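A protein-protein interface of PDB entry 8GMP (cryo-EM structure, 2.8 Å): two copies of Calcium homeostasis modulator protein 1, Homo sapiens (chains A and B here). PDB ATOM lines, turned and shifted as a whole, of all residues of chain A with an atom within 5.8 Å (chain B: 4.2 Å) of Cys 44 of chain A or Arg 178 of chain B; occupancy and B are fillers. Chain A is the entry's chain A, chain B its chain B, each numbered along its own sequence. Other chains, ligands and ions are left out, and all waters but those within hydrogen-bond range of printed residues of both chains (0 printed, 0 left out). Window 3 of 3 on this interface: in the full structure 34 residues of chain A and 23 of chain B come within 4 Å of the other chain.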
ATOM      1  N   ASN A  41      30.229  20.772  21.437  1.00  0.00           N
ATOM      2  CA  ASN A  41      29.631  22.042  21.041  1.00  0.00           C
ATOM      3  C   ASN A  41      29.506  22.895  22.289  1.00  0.00           C
ATOM      4  O   ASN A  41      29.017  22.416  23.315  1.00  0.00           O
ATOM      5  CB  ASN A  41      28.268  21.843  20.369  1.00  0.00           C
ATOM      6  CG  ASN A  41      27.210  21.318  21.321  1.00  0.00           C
ATOM      7  OD1 ASN A  41      27.269  20.173  21.766  1.00  0.00           O
ATOM      8  ND2 ASN A  41      26.243  22.166  21.652  1.00  0.00           N
ATOM      9  N   CYS A  42      29.962  24.116  22.224  1.00  0.00           N
ATOM     10  CA  CYS A  42      29.757  24.641  23.557  1.00  0.00           C
ATOM     11  C   CYS A  42      28.739  25.777  23.538  1.00  0.00           C
ATOM     12  O   CYS A  42      28.401  26.292  22.471  1.00  0.00           O
ATOM     13  CB  CYS A  42      31.087  25.104  24.159  1.00  0.00           C
ATOM     14  SG  CYS A  42      31.682  26.761  23.801  1.00  0.00           S
ATOM     15  N   PRO A  43      28.210  26.181  24.695  1.00  0.00           N
ATOM     16  CA  PRO A  43      27.056  27.094  24.690  1.00  0.00           C
ATOM     17  C   PRO A  43      27.363  28.482  24.165  1.00  0.00           C
ATOM     18  O   PRO A  43      26.457  29.136  23.638  1.00  0.00           O
ATOM     19  CB  PRO A  43      26.644  27.147  26.167  1.00  0.00           C
ATOM     20  CG  PRO A  43      27.336  26.003  26.815  1.00  0.00           C
ATOM     21  CD  PRO A  43      28.594  25.800  26.062  1.00  0.00           C
ATOM     22  N   CYS A  44      28.606  28.939  24.283  1.00  0.00           N
ATOM     23  CA  CYS A  44      29.000  30.338  24.109  1.00  0.00           C
ATOM     24  C   CYS A  44      28.019  31.278  24.811  1.00  0.00           C
ATOM     25  O   CYS A  44      27.349  32.110  24.203  1.00  0.00           O
ATOM     26  CB  CYS A  44      29.218  30.715  22.635  1.00  0.00           C
ATOM     27  SG  CYS A  44      28.190  30.043  21.319  1.00  0.00           S
ATOM     28  N   LEU A  45      27.964  31.120  26.125  1.00  0.00           N
ATOM     29  CA  LEU A  45      27.256  31.999  27.046  1.00  0.00           C
ATOM     30  C   LEU A  45      28.176  32.340  28.200  1.00  0.00           C
ATOM     31  O   LEU A  45      28.978  31.508  28.640  1.00  0.00           O
ATOM     32  CB  LEU A  45      25.971  31.337  27.569  1.00  0.00           C
ATOM     33  CG  LEU A  45      24.724  31.485  26.700  1.00  0.00           C
ATOM     34  CD1 LEU A  45      23.841  30.268  26.844  1.00  0.00           C
ATOM     35  CD2 LEU A  45      23.974  32.742  27.079  1.00  0.00           C
ATOM     36  N   PRO A  46      28.075  33.556  28.740  1.00  0.00           N
ATOM     37  CA  PRO A  46      29.149  34.048  29.621  1.00  0.00           C
ATOM     38  C   PRO A  46      29.246  33.350  30.967  1.00  0.00           C
ATOM     39  O   PRO A  46      30.140  33.686  31.751  1.00  0.00           O
ATOM     40  CB  PRO A  46      28.810  35.535  29.787  1.00  0.00           C
ATOM     41  CG  PRO A  46      27.378  35.657  29.413  1.00  0.00           C
ATOM     42  CD  PRO A  46      27.121  34.616  28.382  1.00  0.00           C
ATOM     43  N   ASN A  49      30.034  28.583  29.890  1.00  0.00           N
ATOM     44  CA  ASN A  49      31.223  28.159  29.159  1.00  0.00           C
ATOM     45  C   ASN A  49      32.166  27.360  30.050  1.00  0.00           C
ATOM     46  O   ASN A  49      32.595  26.256  29.699  1.00  0.00           O
ATOM     47  CB  ASN A  49      31.935  29.387  28.586  1.00  0.00           C
ATOM     48  CG  ASN A  49      31.440  29.759  27.207  1.00  0.00           C
ATOM     49  OD1 ASN A  49      30.597  29.076  26.636  1.00  0.00           O
ATOM     50  ND2 ASN A  49      31.965  30.845  26.666  1.00  0.00           N
ATOM     51  N   CYS A 127      36.791  27.354  24.760  1.00  0.00           N
ATOM     52  CA  CYS A 127      35.496  27.783  25.271  1.00  0.00           C
ATOM     53  C   CYS A 127      35.547  28.246  26.720  1.00  0.00           C
ATOM     54  O   CYS A 127      34.884  29.227  27.059  1.00  0.00           O
ATOM     55  CB  CYS A 127      34.464  26.660  25.120  1.00  0.00           C
ATOM     56  SG  CYS A 127      32.759  27.176  25.478  1.00  0.00           S
ATOM     57  N   ALA A 157      32.265  35.848  24.658  1.00  0.00           N
ATOM     58  CA  ALA A 157      31.846  34.469  24.874  1.00  0.00           C
ATOM     59  C   ALA A 157      31.445  33.757  23.590  1.00  0.00           C
ATOM     60  O   ALA A 157      31.339  32.527  23.601  1.00  0.00           O
ATOM     61  CB  ALA A 157      30.693  34.427  25.872  1.00  0.00           C
ATOM     62  N   ARG A 158      31.230  34.483  22.491  1.00  0.00           N
ATOM     63  CA  ARG A 158      30.789  33.893  21.232  1.00  0.00           C
ATOM     64  C   ARG A 158      31.938  33.624  20.271  1.00  0.00           C
ATOM     65  O   ARG A 158      31.698  33.305  19.102  1.00  0.00           O
ATOM     66  CB  ARG A 158      29.749  34.789  20.563  1.00  0.00           C
ATOM     67  CG  ARG A 158      28.568  35.150  21.439  1.00  0.00           C
ATOM     68  CD  ARG A 158      27.518  35.891  20.637  1.00  0.00           C
ATOM     69  NE  ARG A 158      26.608  36.648  21.487  1.00  0.00           N
ATOM     70  CZ  ARG A 158      26.572  37.974  21.548  1.00  0.00           C
ATOM     71  NH1 ARG A 158      27.397  38.694  20.804  1.00  0.00           N
ATOM     72  NH2 ARG A 158      25.711  38.581  22.350  1.00  0.00           N
ATOM     73  N   VAL A 159      33.178  33.749  20.735  1.00  0.00           N
ATOM     74  CA  VAL A 159      34.365  33.513  19.918  1.00  0.00           C
ATOM     75  C   VAL A 159      34.401  32.080  19.396  1.00  0.00           C
ATOM     76  O   VAL A 159      34.665  31.877  18.203  1.00  0.00           O
ATOM     77  CB  VAL A 159      35.645  33.836  20.707  1.00  0.00           C
ATOM     78  CG1 VAL A 159      36.859  33.284  19.990  1.00  0.00           C
ATOM     79  CG2 VAL A 159      35.776  35.331  20.914  1.00  0.00           C
ATOM     80  N   PRO A 160      34.166  31.056  20.224  1.00  0.00           N
ATOM     81  CA  PRO A 160      34.203  29.686  19.688  1.00  0.00           C
ATOM     82  C   PRO A 160      33.053  29.358  18.751  1.00  0.00           C
ATOM     83  O   PRO A 160      33.085  28.306  18.104  1.00  0.00           O
ATOM     84  CB  PRO A 160      34.167  28.811  20.950  1.00  0.00           C
ATOM     85  CG  PRO A 160      33.708  29.698  22.036  1.00  0.00           C
ATOM     86  CD  PRO A 160      34.177  31.058  21.697  1.00  0.00           C
ATOM     87  N   CYS A 161      32.041  30.215  18.654  1.00  0.00           N
ATOM     88  CA  CYS A 161      30.905  29.971  17.774  1.00  0.00           C
ATOM     89  C   CYS A 161      30.976  30.925  16.585  1.00  0.00           C
ATOM     90  O   CYS A 161      30.671  32.115  16.723  1.00  0.00           O
ATOM     91  CB  CYS A 161      29.592  30.122  18.551  1.00  0.00           C
ATOM     92  SG  CYS A 161      29.532  29.133  20.089  1.00  0.00           S
ATOM     93  N   PRO A 162      31.386  30.441  15.404  1.00  0.00           N
ATOM     94  CA  PRO A 162      31.665  31.348  14.280  1.00  0.00           C
ATOM     95  C   PRO A 162      30.436  32.012  13.679  1.00  0.00           C
ATOM     96  O   PRO A 162      30.528  33.120  13.144  1.00  0.00           O
ATOM     97  CB  PRO A 162      32.345  30.433  13.252  1.00  0.00           C
ATOM     98  CG  PRO A 162      31.975  29.059  13.641  1.00  0.00           C
ATOM     99  CD  PRO A 162      31.800  29.059  15.119  1.00  0.00           C
ATOM    100  N   GLU A 163      29.284  31.345  13.745  1.00  0.00           N
ATOM    101  CA  GLU A 163      28.070  31.897  13.153  1.00  0.00           C
ATOM    102  C   GLU A 163      27.364  32.873  14.085  1.00  0.00           C
ATOM    103  O   GLU A 163      26.541  33.668  13.622  1.00  0.00           O
ATOM    104  CB  GLU A 163      27.119  30.767  12.765  1.00  0.00           C
ATOM    105  CG  GLU A 163      26.590  29.970  13.950  1.00  0.00           C
ATOM    106  CD  GLU A 163      27.519  28.841  14.358  1.00  0.00           C
ATOM    107  OE1 GLU A 163      28.544  28.635  13.677  1.00  0.00           O
ATOM    108  OE2 GLU A 163      27.229  28.164  15.365  1.00  0.00           O
ATOM    109  N   ILE A 164      27.661  32.828  15.385  1.00  0.00           N
ATOM    110  CA  ILE A 164      27.051  33.723  16.359  1.00  0.00           C
ATOM    111  C   ILE A 164      27.885  34.969  16.606  1.00  0.00           C
ATOM    112  O   ILE A 164      27.353  35.975  17.091  1.00  0.00           O
ATOM    113  CB  ILE A 164      26.803  32.992  17.695  1.00  0.00           C
ATOM    114  CG1 ILE A 164      26.148  31.635  17.458  1.00  0.00           C
ATOM    115  CG2 ILE A 164      25.930  33.831  18.608  1.00  0.00           C
ATOM    116  CD1 ILE A 164      25.731  30.946  18.733  1.00  0.00           C
ATOM    117  N   GLU B 174      20.000  29.301  16.257  1.00  0.00           N
ATOM    118  CA  GLU B 174      21.197  28.625  16.732  1.00  0.00           C
ATOM    119  C   GLU B 174      21.586  29.045  18.144  1.00  0.00           C
ATOM    120  O   GLU B 174      22.513  28.467  18.719  1.00  0.00           O
ATOM    121  CB  GLU B 174      22.358  28.864  15.764  1.00  0.00           C
ATOM    122  CG  GLU B 174      23.536  27.933  15.988  1.00  0.00           C
ATOM    123  CD  GLU B 174      23.208  26.493  15.639  1.00  0.00           C
ATOM    124  OE1 GLU B 174      22.296  26.270  14.816  1.00  0.00           O
ATOM    125  OE2 GLU B 174      23.863  25.581  16.185  1.00  0.00           O
ATOM    126  N   ALA B 176      18.945  29.187  20.565  1.00  0.00           N
ATOM    127  CA  ALA B 176      18.085  28.273  21.307  1.00  0.00           C
ATOM    128  C   ALA B 176      18.548  26.832  21.156  1.00  0.00           C
ATOM    129  O   ALA B 176      18.597  26.088  22.138  1.00  0.00           O
ATOM    130  CB  ALA B 176      16.635  28.413  20.845  1.00  0.00           C
ATOM    131  N   VAL B 177      18.887  26.420  19.937  1.00  0.00           N
ATOM    132  CA  VAL B 177      19.741  25.257  19.740  1.00  0.00           C
ATOM    133  C   VAL B 177      21.095  25.656  20.306  1.00  0.00           C
ATOM    134  O   VAL B 177      21.369  26.849  20.475  1.00  0.00           O
ATOM    135  CB  VAL B 177      19.834  24.856  18.257  1.00  0.00           C
ATOM    136  CG1 VAL B 177      20.538  23.525  18.103  1.00  0.00           C
ATOM    137  CG2 VAL B 177      18.455  24.805  17.638  1.00  0.00           C
ATOM    138  N   ARG B 178      21.933  24.676  20.644  1.00  0.00           N
ATOM    139  CA  ARG B 178      23.257  24.903  21.230  1.00  0.00           C
ATOM    140  C   ARG B 178      23.176  25.337  22.693  1.00  0.00           C
ATOM    141  O   ARG B 178      24.191  25.392  23.385  1.00  0.00           O
ATOM    142  CB  ARG B 178      24.058  25.927  20.411  1.00  0.00           C
ATOM    143  CG  ARG B 178      25.498  26.120  20.825  1.00  0.00           C
ATOM    144  CD  ARG B 178      26.153  27.197  19.986  1.00  0.00           C
ATOM    145  NE  ARG B 178      26.640  26.688  18.710  1.00  0.00           N
ATOM    146  CZ  ARG B 178      27.836  26.139  18.534  1.00  0.00           C
ATOM    147  NH1 ARG B 178      28.671  26.022  19.554  1.00  0.00           N
ATOM    148  NH2 ARG B 178      28.200  25.705  17.337  1.00  0.00           N
ATOM    149  N   TYR B 179      21.973  25.619  23.185  1.00  0.00           N
ATOM    150  CA  TYR B 179      21.721  25.793  24.609  1.00  0.00           C
ATOM    151  C   TYR B 179      20.894  24.670  25.207  1.00  0.00           C
ATOM    152  O   TYR B 179      21.102  24.335  26.376  1.00  0.00           O
ATOM    153  CB  TYR B 179      21.017  27.134  24.863  1.00  0.00           C
ATOM    154  CG  TYR B 179      20.394  27.292  26.230  1.00  0.00           C
ATOM    155  CD1 TYR B 179      21.154  27.692  27.315  1.00  0.00           C
ATOM    156  CD2 TYR B 179      19.040  27.074  26.430  1.00  0.00           C
ATOM    157  CE1 TYR B 179      20.591  27.847  28.561  1.00  0.00           C
ATOM    158  CE2 TYR B 179      18.470  27.223  27.673  1.00  0.00           C
ATOM    159  CZ  TYR B 179      19.249  27.612  28.735  1.00  0.00           C
ATOM    160  OH  TYR B 179      18.685  27.766  29.978  1.00  0.00           O
ATOM    161  N   LEU B 180      19.973  24.069  24.453  1.00  0.00           N
ATOM    162  CA  LEU B 180      19.261  22.873  24.865  1.00  0.00           C
ATOM    163  C   LEU B 180      20.063  21.604  24.630  1.00  0.00           C
ATOM    164  O   LEU B 180      19.797  20.593  25.283  1.00  0.00           O
ATOM    165  CB  LEU B 180      17.924  22.766  24.119  1.00  0.00           C
ATOM    166  CG  LEU B 180      16.848  23.800  24.445  1.00  0.00           C
ATOM    167  CD1 LEU B 180      15.807  23.822  23.350  1.00  0.00           C
ATOM    168  CD2 LEU B 180      16.208  23.505  25.784  1.00  0.00           C
ATOM    169  N   CYS B 182      23.218  21.444  25.331  1.00  0.00           N
ATOM    170  CA  CYS B 182      24.224  21.384  26.384  1.00  0.00           C
ATOM    171  C   CYS B 182      23.614  20.892  27.690  1.00  0.00           C
ATOM    172  O   CYS B 182      24.267  20.189  28.465  1.00  0.00           O
ATOM    173  CB  CYS B 182      24.881  22.753  26.569  1.00  0.00           C
ATOM    174  SG  CYS B 182      25.951  23.237  25.205  1.00  0.00           S
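The side-chain sulfur of Cys 182 of chain B sits at hydrogen-bond distance from the backbone carbonyl oxygen of Asn 41 of chain A (3.7 Å).
O of Cys 42 of chain A is in hydrogen-bond range of NH1 of Arg 178 of chain B, 2.9 Å away.
SG of Cys 161 of chain A is in hydrogen-bond range of NH1 of Arg 178 of chain B (3.3 Å).
NH2 of Arg 178 of chain B is in salt-bridge range of OE2 of Glu 163 of chain A (3.3 Å).
The backbone nitrogen (N) of Pro 43 of chain A sits close to the side-chain sulfur (SG) of Cys 182 of chain B, at 3.7 Å.
The side-chain sulfur of Cys 42 of chain A is disulfide-bonded to the side-chain sulfur of Cys 127 of chain A (2.0 Å).
OD1 of Asn 49 of chain A sits at hydrogen-bond distance from N of Cys 44 of chain A, at 3.1 Å.
SG of Cys 44 of chain A forms a disulfide with SG of Cys 161 of chain A (2.0 Å).
The side-chain amide oxygen (OD1) of Asn 49 of chain A is in hydrogen-bond range of the backbone NH (N) of Leu 45 of chain A.
The side-chain carboxylate (OE2) of Glu 174 of chain B is in salt-bridge range of the guanidinium group (NE) of Arg 178 of chain B.
The backbone carbonyl oxygen (O) of Arg 178 of chain B is in hydrogen-bond range of the side-chain sulfur (SG) of Cys 182 of chain B, 3.3 Å away.
Among the printed residues, merely in contact across the chains: Pro 43 of chain A with Arg 178 of chain B (3.6 Å), Cys 44 of chain A with Arg 178 of chain B (3.7 Å), Leu 45 of chain A with Tyr 179 of chain B (3.8 Å), Glu 163 of chain A with Glu 174 of chain B (3.8 Å) and Ile 164 of chain A with Arg 178 of chain B (3.98 Å).
Of chain B, only Arg 178 comes within 4 Å of Cys 44 of chain A.
Of the printed residues of chain B, Leu 45 of chain A touches Tyr 179 (3.8 Å).
Cys 127 of chain A touches none of the printed residues of chain B.
Arg 178 of chain B touches just these residues of chain A: Cys 42, Pro 43, Cys 44, Cys 161, Glu 163 and Ile 164.
Printed residues of chain A within 4 Å of Cys 182 of chain B: Asn 41 and Pro 43.
The nearest printed residue of chain B that does not touch Cys 44 of chain A is Cys 182 of chain B (6.4 Å).
The nearest printed residue of chain B that does not touch Pro 43 of chain A is Tyr 179 of chain B (5.3 Å).
Printed residues of chain B that touch a printed residue of chain A: Glu 174, Arg 178, Tyr 179 and Cys 182.
Hydrophobic or aromatic side chains of chain B within 4 Å of the printed part of chain A: Tyr 179.
Among the printed residues, 10 pairs touch across the chains.
Among the printed residues, Asp or Glu carboxylates within 4 Å of a Lys or Arg side-chain nitrogen of the other chain: Glu 163 of chain A with Arg 178 of chain B (3.3 Å).
No position is printed for both chains.
Of the 10 pairs that touch across the chains among the printed residues, none has its exchanged pair printed and touching as well.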
